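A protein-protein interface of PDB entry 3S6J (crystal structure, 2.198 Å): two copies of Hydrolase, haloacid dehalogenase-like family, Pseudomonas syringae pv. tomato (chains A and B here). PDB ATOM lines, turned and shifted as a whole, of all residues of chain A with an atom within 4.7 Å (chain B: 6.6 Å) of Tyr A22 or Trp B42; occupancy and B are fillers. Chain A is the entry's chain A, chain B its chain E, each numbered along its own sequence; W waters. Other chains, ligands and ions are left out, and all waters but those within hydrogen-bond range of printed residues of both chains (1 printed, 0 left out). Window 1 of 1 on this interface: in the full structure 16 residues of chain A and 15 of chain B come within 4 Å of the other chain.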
ATOM      1  N   ASP A  19      24.783 -17.766  11.352  1.00  0.00           N
ATOM      2  CA  ASP A  19      24.436 -16.412  11.002  1.00  0.00           C
ATOM      3  C   ASP A  19      25.723 -15.676  10.680  1.00  0.00           C
ATOM      4  O   ASP A  19      26.260 -14.961  11.528  1.00  0.00           O
ATOM      5  CB  ASP A  19      23.710 -15.736  12.166  1.00  0.00           C
ATOM      6  CG  ASP A  19      23.276 -14.319  11.837  1.00  0.00           C
ATOM      7  OD1 ASP A  19      23.356 -13.917  10.644  1.00  0.00           O
ATOM      8  OD2 ASP A  19      22.855 -13.609  12.771  1.00  0.00           O
ATOM      9  N   SER A  20      26.208 -15.864   9.450  1.00  0.00           N
ATOM     10  CA  SER A  20      27.519 -15.358   9.041  1.00  0.00           C
ATOM     11  C   SER A  20      27.494 -14.607   7.727  1.00  0.00           C
ATOM     12  O   SER A  20      28.537 -14.112   7.290  1.00  0.00           O
ATOM     13  CB  SER A  20      28.516 -16.504   8.895  1.00  0.00           C
ATOM     14  OG  SER A  20      27.879 -17.649   8.365  1.00  0.00           O
ATOM     15  N   VAL A  21      26.327 -14.536   7.081  1.00  0.00           N
ATOM     16  CA  VAL A  21      26.274 -13.844   5.793  1.00  0.00           C
ATOM     17  C   VAL A  21      26.712 -12.385   5.925  1.00  0.00           C
ATOM     18  O   VAL A  21      27.432 -11.882   5.096  1.00  0.00           O
ATOM     19  CB  VAL A  21      24.895 -13.920   5.132  1.00  0.00           C
ATOM     20  CG1 VAL A  21      24.776 -12.860   4.054  1.00  0.00           C
ATOM     21  CG2 VAL A  21      24.660 -15.306   4.554  1.00  0.00           C
ATOM     22  N   TYR A  22      26.298 -11.712   6.987  1.00  0.00           N
ATOM     23  CA  TYR A  22      26.714 -10.333   7.173  1.00  0.00           C
ATOM     24  C   TYR A  22      28.213 -10.175   7.472  1.00  0.00           C
ATOM     25  O   TYR A  22      28.829  -9.165   7.112  1.00  0.00           O
ATOM     26  CB  TYR A  22      25.822  -9.654   8.197  1.00  0.00           C
ATOM     27  CG  TYR A  22      24.395  -9.538   7.691  1.00  0.00           C
ATOM     28  CD1 TYR A  22      23.550 -10.646   7.674  1.00  0.00           C
ATOM     29  CD2 TYR A  22      23.905  -8.336   7.189  1.00  0.00           C
ATOM     30  CE1 TYR A  22      22.249 -10.551   7.210  1.00  0.00           C
ATOM     31  CE2 TYR A  22      22.610  -8.231   6.727  1.00  0.00           C
ATOM     32  CZ  TYR A  22      21.787  -9.350   6.728  1.00  0.00           C
ATOM     33  OH  TYR A  22      20.500  -9.281   6.231  1.00  0.00           O
ATOM     34  N   GLN A  23      28.817 -11.174   8.103  1.00  0.00           N
ATOM     35  CA  GLN A  23      30.246 -11.084   8.352  1.00  0.00           C
ATOM     36  C   GLN A  23      30.955 -11.308   7.032  1.00  0.00           C
ATOM     37  O   GLN A  23      31.989 -10.720   6.764  1.00  0.00           O
ATOM     38  CB  GLN A  23      30.723 -12.109   9.392  1.00  0.00           C
ATOM     39  CG  GLN A  23      30.497 -11.699  10.849  1.00  0.00           C
ATOM     40  CD  GLN A  23      29.032 -11.708  11.217  1.00  0.00           C
ATOM     41  OE1 GLN A  23      28.216 -12.315  10.521  1.00  0.00           O
ATOM     42  NE2 GLN A  23      28.686 -11.044  12.315  1.00  0.00           N
ATOM     43  N   ASN A  24      30.381 -12.175   6.210  1.00  0.00           N
ATOM     44  CA  ASN A  24      30.943 -12.487   4.913  1.00  0.00           C
ATOM     45  C   ASN A  24      30.913 -11.252   4.018  1.00  0.00           C
ATOM     46  O   ASN A  24      31.902 -10.914   3.402  1.00  0.00           O
ATOM     47  CB  ASN A  24      30.190 -13.648   4.286  1.00  0.00           C
ATOM     48  CG  ASN A  24      31.014 -14.396   3.303  1.00  0.00           C
ATOM     49  OD1 ASN A  24      31.951 -13.843   2.706  1.00  0.00           O
ATOM     50  ND2 ASN A  24      30.674 -15.663   3.097  1.00  0.00           N
ATOM     51  N   VAL A  25      29.776 -10.564   4.000  1.00  0.00           N
ATOM     52  CA  VAL A  25      29.639  -9.301   3.288  1.00  0.00           C
ATOM     53  C   VAL A  25      30.692  -8.289   3.764  1.00  0.00           C
ATOM     54  O   VAL A  25      31.353  -7.631   2.959  1.00  0.00           O
ATOM     55  CB  VAL A  25      28.215  -8.717   3.473  1.00  0.00           C
ATOM     56  CG1 VAL A  25      28.130  -7.307   2.915  1.00  0.00           C
ATOM     57  CG2 VAL A  25      27.169  -9.619   2.790  1.00  0.00           C
ATOM     58  N   ALA A  26      30.850  -8.178   5.075  1.00  0.00           N
ATOM     59  CA  ALA A  26      31.760  -7.203   5.670  1.00  0.00           C
ATOM     60  C   ALA A  26      33.226  -7.509   5.376  1.00  0.00           C
ATOM     61  O   ALA A  26      34.033  -6.593   5.263  1.00  0.00           O
ATOM     62  CB  ALA A  26      31.524  -7.101   7.184  1.00  0.00           C
ATOM     63  N   HIS A  45      26.240  -8.439  -1.123  1.00  0.00           N
ATOM     64  CA  HIS A  45      25.299  -9.329  -0.434  1.00  0.00           C
ATOM     65  C   HIS A  45      24.594 -10.265  -1.432  1.00  0.00           C
ATOM     66  O   HIS A  45      24.489 -11.468  -1.210  1.00  0.00           O
ATOM     67  CB  HIS A  45      24.306  -8.481   0.375  1.00  0.00           C
ATOM     68  CG  HIS A  45      23.455  -9.260   1.330  1.00  0.00           C
ATOM     69  ND1 HIS A  45      22.606  -8.653   2.225  1.00  0.00           N
ATOM     70  CD2 HIS A  45      23.337 -10.595   1.539  1.00  0.00           C
ATOM     71  CE1 HIS A  45      21.983  -9.579   2.934  1.00  0.00           C
ATOM     72  NE2 HIS A  45      22.395 -10.763   2.521  1.00  0.00           N
ATOM     73  N   LEU A 191      15.158 -17.529   5.104  1.00  0.00           N
ATOM     74  CA  LEU A 191      15.257 -16.070   5.081  1.00  0.00           C
ATOM     75  C   LEU A 191      16.497 -15.546   5.830  1.00  0.00           C
ATOM     76  O   LEU A 191      16.819 -14.358   5.760  1.00  0.00           O
ATOM     77  CB  LEU A 191      14.007 -15.448   5.707  1.00  0.00           C
ATOM     78  CG  LEU A 191      12.672 -15.581   4.961  1.00  0.00           C
ATOM     79  CD1 LEU A 191      11.547 -14.797   5.676  1.00  0.00           C
ATOM     80  CD2 LEU A 191      12.814 -15.102   3.542  1.00  0.00           C
ATOM     81  N   SER A 192      17.177 -16.449   6.533  1.00  0.00           N
ATOM     82  CA  SER A 192      18.190 -16.088   7.527  1.00  0.00           C
ATOM     83  C   SER A 192      19.488 -15.611   6.878  1.00  0.00           C
ATOM     84  O   SER A 192      20.453 -15.253   7.558  1.00  0.00           O
ATOM     85  CB  SER A 192      18.436 -17.288   8.442  1.00  0.00           C
ATOM     86  OG  SER A 192      18.768 -18.435   7.672  1.00  0.00           O
ATOM     87  N   GLY A 193      19.503 -15.597   5.544  1.00  0.00           N
ATOM     88  CA  GLY A 193      20.657 -15.121   4.792  1.00  0.00           C
ATOM     89  C   GLY A 193      20.398 -13.713   4.285  1.00  0.00           C
ATOM     90  O   GLY A 193      21.240 -13.106   3.632  1.00  0.00           O
ATOM     91  N   GLY A 194      19.229 -13.177   4.616  1.00  0.00           N
ATOM     92  CA  GLY A 194      18.844 -11.875   4.111  1.00  0.00           C
ATOM     93  C   GLY A 194      18.293 -11.832   2.682  1.00  0.00           C
ATOM     94  O   GLY A 194      18.063 -10.753   2.197  1.00  0.00           O
ATOM     95  N   GLU A 210      11.710 -19.185   7.738  1.00  0.00           N
ATOM     96  CA  GLU A 210      12.457 -18.104   8.348  1.00  0.00           C
ATOM     97  C   GLU A 210      13.893 -18.500   8.634  1.00  0.00           C
ATOM     98  O   GLU A 210      14.804 -17.751   8.326  1.00  0.00           O
ATOM     99  CB  GLU A 210      11.777 -17.656   9.643  1.00  0.00           C
ATOM    100  CG  GLU A 210      10.370 -17.092   9.420  1.00  0.00           C
ATOM    101  CD  GLU A 210       9.874 -16.300  10.625  1.00  0.00           C
ATOM    102  OE1 GLU A 210      10.437 -16.480  11.729  1.00  0.00           O
ATOM    103  OE2 GLU A 210       8.933 -15.488  10.470  1.00  0.00           O
ATOM    104  N   TYR B  22      24.147  -1.452   6.346  1.00  0.00           N
ATOM    105  CA  TYR B  22      24.885  -2.576   6.883  1.00  0.00           C
ATOM    106  C   TYR B  22      25.691  -2.174   8.126  1.00  0.00           C
ATOM    107  O   TYR B  22      25.920  -2.996   9.028  1.00  0.00           O
ATOM    108  CB  TYR B  22      25.763  -3.232   5.790  1.00  0.00           C
ATOM    109  CG  TYR B  22      24.914  -3.954   4.749  1.00  0.00           C
ATOM    110  CD1 TYR B  22      24.218  -3.239   3.771  1.00  0.00           C
ATOM    111  CD2 TYR B  22      24.775  -5.343   4.762  1.00  0.00           C
ATOM    112  CE1 TYR B  22      23.430  -3.885   2.825  1.00  0.00           C
ATOM    113  CE2 TYR B  22      23.976  -5.991   3.822  1.00  0.00           C
ATOM    114  CZ  TYR B  22      23.307  -5.253   2.863  1.00  0.00           C
ATOM    115  OH  TYR B  22      22.499  -5.884   1.948  1.00  0.00           O
ATOM    116  N   VAL B  25      22.871  -2.072  10.791  1.00  0.00           N
ATOM    117  CA  VAL B  25      22.669  -3.450  11.234  1.00  0.00           C
ATOM    118  C   VAL B  25      23.731  -3.921  12.245  1.00  0.00           C
ATOM    119  O   VAL B  25      23.399  -4.449  13.309  1.00  0.00           O
ATOM    120  CB  VAL B  25      22.593  -4.447  10.029  1.00  0.00           C
ATOM    121  CG1 VAL B  25      22.339  -5.855  10.527  1.00  0.00           C
ATOM    122  CG2 VAL B  25      21.486  -4.057   9.081  1.00  0.00           C
ATOM    123  N   LEU B  39      19.605 -11.798  18.405  1.00  0.00           N
ATOM    124  CA  LEU B  39      18.670 -11.759  17.288  1.00  0.00           C
ATOM    125  C   LEU B  39      19.502 -11.943  16.046  1.00  0.00           C
ATOM    126  O   LEU B  39      20.532 -11.289  15.913  1.00  0.00           O
ATOM    127  CB  LEU B  39      18.002 -10.394  17.221  1.00  0.00           C
ATOM    128  CG  LEU B  39      16.491 -10.472  17.123  1.00  0.00           C
ATOM    129  CD1 LEU B  39      15.883 -10.302  18.506  1.00  0.00           C
ATOM    130  CD2 LEU B  39      15.981  -9.411  16.162  1.00  0.00           C
ATOM    131  N   ALA B  40      19.086 -12.844  15.159  1.00  0.00           N
ATOM    132  CA  ALA B  40      19.818 -13.052  13.913  1.00  0.00           C
ATOM    133  C   ALA B  40      19.863 -11.736  13.145  1.00  0.00           C
ATOM    134  O   ALA B  40      18.941 -10.925  13.198  1.00  0.00           O
ATOM    135  CB  ALA B  40      19.179 -14.158  13.070  1.00  0.00           C
ATOM    136  N   MET B  41      20.942 -11.494  12.432  1.00  0.00           N
ATOM    137  CA  MET B  41      21.039 -10.215  11.741  1.00  0.00           C
ATOM    138  C   MET B  41      20.027  -9.933  10.627  1.00  0.00           C
ATOM    139  O   MET B  41      19.731  -8.777  10.371  1.00  0.00           O
ATOM    140  CB  MET B  41      22.474  -9.943  11.300  1.00  0.00           C
ATOM    141  CG  MET B  41      23.182  -9.123  12.383  1.00  0.00           C
ATOM    142  SD  MET B  41      24.988  -9.247  12.133  1.00  0.00           S
ATOM    143  CE  MET B  41      25.316  -7.469  11.361  1.00  0.00           C
ATOM    144  N   TRP B  42      19.477 -10.956   9.988  1.00  0.00           N
ATOM    145  CA  TRP B  42      18.428 -10.706   8.985  1.00  0.00           C
ATOM    146  C   TRP B  42      17.167 -10.046   9.607  1.00  0.00           C
ATOM    147  O   TRP B  42      16.541  -9.173   8.979  1.00  0.00           O
ATOM    148  CB  TRP B  42      18.063 -11.982   8.215  1.00  0.00           C
ATOM    149  CG  TRP B  42      17.219 -12.937   9.013  1.00  0.00           C
ATOM    150  CD1 TRP B  42      17.652 -13.827   9.954  1.00  0.00           C
ATOM    151  CD2 TRP B  42      15.796 -13.096   8.933  1.00  0.00           C
ATOM    152  NE1 TRP B  42      16.575 -14.527  10.471  1.00  0.00           N
ATOM    153  CE2 TRP B  42      15.432 -14.093   9.857  1.00  0.00           C
ATOM    154  CE3 TRP B  42      14.798 -12.482   8.173  1.00  0.00           C
ATOM    155  CZ2 TRP B  42      14.104 -14.485  10.056  1.00  0.00           C
ATOM    156  CZ3 TRP B  42      13.487 -12.878   8.358  1.00  0.00           C
ATOM    157  CH2 TRP B  42      13.154 -13.873   9.295  1.00  0.00           C
ATOM    158  N   ARG B  43      16.818 -10.446  10.836  1.00  0.00           N
ATOM    159  CA  ARG B  43      15.685  -9.863  11.565  1.00  0.00           C
ATOM    160  C   ARG B  43      15.936  -8.394  11.904  1.00  0.00           C
ATOM    161  O   ARG B  43      15.020  -7.583  11.872  1.00  0.00           O
ATOM    162  CB  ARG B  43      15.353 -10.661  12.860  1.00  0.00           C
ATOM    163  CG  ARG B  43      15.368 -12.188  12.705  1.00  0.00           C
ATOM    164  CD  ARG B  43      14.618 -12.943  13.813  1.00  0.00           C
ATOM    165  NE  ARG B  43      13.187 -12.897  13.515  1.00  0.00           N
ATOM    166  CZ  ARG B  43      12.420 -13.946  13.235  1.00  0.00           C
ATOM    167  NH1 ARG B  43      12.908 -15.172  13.252  1.00  0.00           N
ATOM    168  NH2 ARG B  43      11.142 -13.751  12.962  1.00  0.00           N
ATOM    169  N   ILE B  44      17.178  -8.049  12.242  1.00  0.00           N
ATOM    170  CA  ILE B  44      17.531  -6.645  12.483  1.00  0.00           C
ATOM    171  C   ILE B  44      17.475  -5.829  11.181  1.00  0.00           C
ATOM    172  O   ILE B  44      16.993  -4.692  11.160  1.00  0.00           O
ATOM    173  CB  ILE B  44      18.925  -6.499  13.148  1.00  0.00           C
ATOM    174  CG1 ILE B  44      18.924  -7.174  14.534  1.00  0.00           C
ATOM    175  CG2 ILE B  44      19.297  -5.017  13.266  1.00  0.00           C
ATOM    176  CD1 ILE B  44      20.306  -7.473  15.132  1.00  0.00           C
ATOM    177  N   HIS B  45      17.943  -6.435  10.095  1.00  0.00           N
ATOM    178  CA  HIS B  45      17.993  -5.779   8.777  1.00  0.00           C
ATOM    179  C   HIS B  45      16.574  -5.471   8.308  1.00  0.00           C
ATOM    180  O   HIS B  45      16.326  -4.443   7.680  1.00  0.00           O
ATOM    181  CB  HIS B  45      18.727  -6.677   7.755  1.00  0.00           C
ATOM    182  CG  HIS B  45      19.048  -6.003   6.449  1.00  0.00           C
ATOM    183  ND1 HIS B  45      19.807  -6.605   5.479  1.00  0.00           N
ATOM    184  CD2 HIS B  45      18.725  -4.768   5.976  1.00  0.00           C
ATOM    185  CE1 HIS B  45      19.950  -5.774   4.454  1.00  0.00           C
ATOM    186  NE2 HIS B  45      19.300  -4.660   4.736  1.00  0.00           N
ATOM    187  N   ARG B  46      15.638  -6.357   8.631  1.00  0.00           N
ATOM    188  CA  ARG B  46      14.232  -6.174   8.252  1.00  0.00           C
ATOM    189  C   ARG B  46      13.621  -4.887   8.812  1.00  0.00           C
ATOM    190  O   ARG B  46      12.701  -4.324   8.218  1.00  0.00           O
ATOM    191  CB  ARG B  46      13.385  -7.351   8.754  1.00  0.00           C
ATOM    192  CG  ARG B  46      13.337  -8.566   7.848  1.00  0.00           C
ATOM    193  CD  ARG B  46      11.983  -9.298   8.011  1.00  0.00           C
ATOM    194  NE  ARG B  46      11.623  -9.579   9.412  1.00  0.00           N
ATOM    195  CZ  ARG B  46      10.761 -10.532   9.791  1.00  0.00           C
ATOM    196  NH1 ARG B  46      10.164 -11.304   8.885  1.00  0.00           N
ATOM    197  NH2 ARG B  46      10.494 -10.722  11.079  1.00  0.00           N
ATOM    198  N   LYS B  47      14.101  -4.444   9.974  1.00  0.00           N
ATOM    199  CA  LYS B  47      13.501  -3.303  10.667  1.00  0.00           C
ATOM    200  C   LYS B  47      14.232  -1.974  10.417  1.00  0.00           C
ATOM    201  O   LYS B  47      13.769  -0.908  10.827  1.00  0.00           O
ATOM    202  CB  LYS B  47      13.445  -3.553  12.181  1.00  0.00           C
ATOM    203  CG  LYS B  47      12.878  -4.903  12.612  1.00  0.00           C
ATOM    204  CD  LYS B  47      11.426  -5.116  12.180  1.00  0.00           C
ATOM    205  CE  LYS B  47      10.786  -6.276  12.957  1.00  0.00           C
ATOM    206  NZ  LYS B  47       9.513  -6.760  12.330  1.00  0.00           N
ATOM    207  N   GLU B  62       8.050  -9.769  18.418  1.00  0.00           N
ATOM    208  CA  GLU B  62       8.257 -10.937  17.560  1.00  0.00           C
ATOM    209  C   GLU B  62       9.082 -12.031  18.244  1.00  0.00           C
ATOM    210  O   GLU B  62       9.079 -13.183  17.808  1.00  0.00           O
ATOM    211  CB  GLU B  62       8.763 -10.559  16.163  1.00  0.00           C
ATOM    212  CG  GLU B  62      10.258 -10.644  15.890  1.00  0.00           C
ATOM    213  CD  GLU B  62      10.565 -10.331  14.417  1.00  0.00           C
ATOM    214  OE1 GLU B  62      11.647 -10.708  13.895  1.00  0.00           O
ATOM    215  OE2 GLU B  62       9.690  -9.710  13.770  1.00  0.00           O
HETATM  216  O   HOH W   1      20.841 -13.434   9.747  1.00  0.00           O
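The backbone carbonyl oxygen (O) of Asp A19 lies close to the side-chain amide oxygen (OE1) of Gln A23 (3.4 Å).
The backbone carbonyl oxygen of Gly A193 lies within hydrogen-bond range of a ring nitrogen (NE2) of His A45 (2.8 Å).
N of Leu A191 is in hydrogen-bond range of O of Glu A210, at 3.2 Å.
The backbone NH (N) of Ser A192 lies within hydrogen-bond range of the backbone carbonyl oxygen (O) of Glu A210 (3.2 Å).
The guanidinium group of Arg B43 is in salt-bridge range of the side-chain carboxylate of Glu B62 (2.7 Å).
Printed residues of chain B within 4 Å of Asp A19: Ala B40 (3.3 Å) and Met B41 (2.9 Å).
Ala A26 touches none of the printed residues of chain B.
Printed residues of chain B within 4 Å of His A45: Tyr B22 (2.8 Å).
Printed residues of chain B within 4 Å of Ser A192: Trp B42 (3.4 Å).
Printed residues of chain B within 4 Å of Gly A194: Trp B42 (3.97 Å).
Of chain A, only Tyr A22 (3.7 Å), Leu A191 (3.6 Å), Ser A192 (3.4 Å), Gly A194 (3.97 Å) and Glu A210 (3.8 Å) come within 4 Å of Trp B42.
Glu B62 touches none of the printed residues of chain A.
The nearest printed residue of chain A that does not touch Trp B42 is Gly A193 (4.7 Å).
Asp A19 touches Ala B40 (OD2 to CA, 3.3 Å).
Tyr B22 touches Tyr A22.
Met B41 touches Tyr A22 (CB to CD1, 3.8 Å).
OH of Tyr A22 touches CA of Trp B42, at 3.7 Å.
CD2 of Trp B42 touches O of Leu A191, at 3.6 Å.
CA of Ser A192 touches CD1 of Trp B42, 3.4 Å away.
CB of Trp B42 touches N of Gly A194, at 3.97 Å.
Glu A210 touches Trp B42.
Tyr B22 touches its own counterpart, Tyr A22.
Tyr A22 touches His B45, and with the chains exchanged His A45 touches Tyr B22.
Water W1 lies within hydrogen-bond range of OD1 of Asp A19 (2.7 Å), N of Trp B42 (2.8 Å), O of Ser A192 (2.9 Å) and N of Met B41 (3.3 Å).
Hydrophobic or aromatic side chains of chain B that line the printed part of chain A: Tyr B22, Ala B40, Met B41, Trp B42 and His B45.
Printed residues of chain A that touch a printed residue of chain B: Asp A19, Tyr A22, His A45, Leu A191, Ser A192, Gly A194 and Glu A210.
Among the printed residues, 12 pairs touch across the chains.
Among the printed residues, Asp or Glu carboxylates within 4 Å of a Lys or Arg side-chain nitrogen of the other chain: Glu A210 with Arg B43.
The side-chain carboxylate (OD2) of Asp A19 is in hydrogen-bond range of the backbone NH (N) of Met B41.
ND1 of His B45 is in hydrogen-bond range of OH of Tyr A22, 2.9 Å away.
A ring nitrogen (ND1) of His A45 is in hydrogen-bond range of the side-chain hydroxyl (OH) of Tyr B22, 2.8 Å away.
NH2 of Arg B43 is in salt-bridge range of OE1 of Glu A210, 3.1 Å away.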
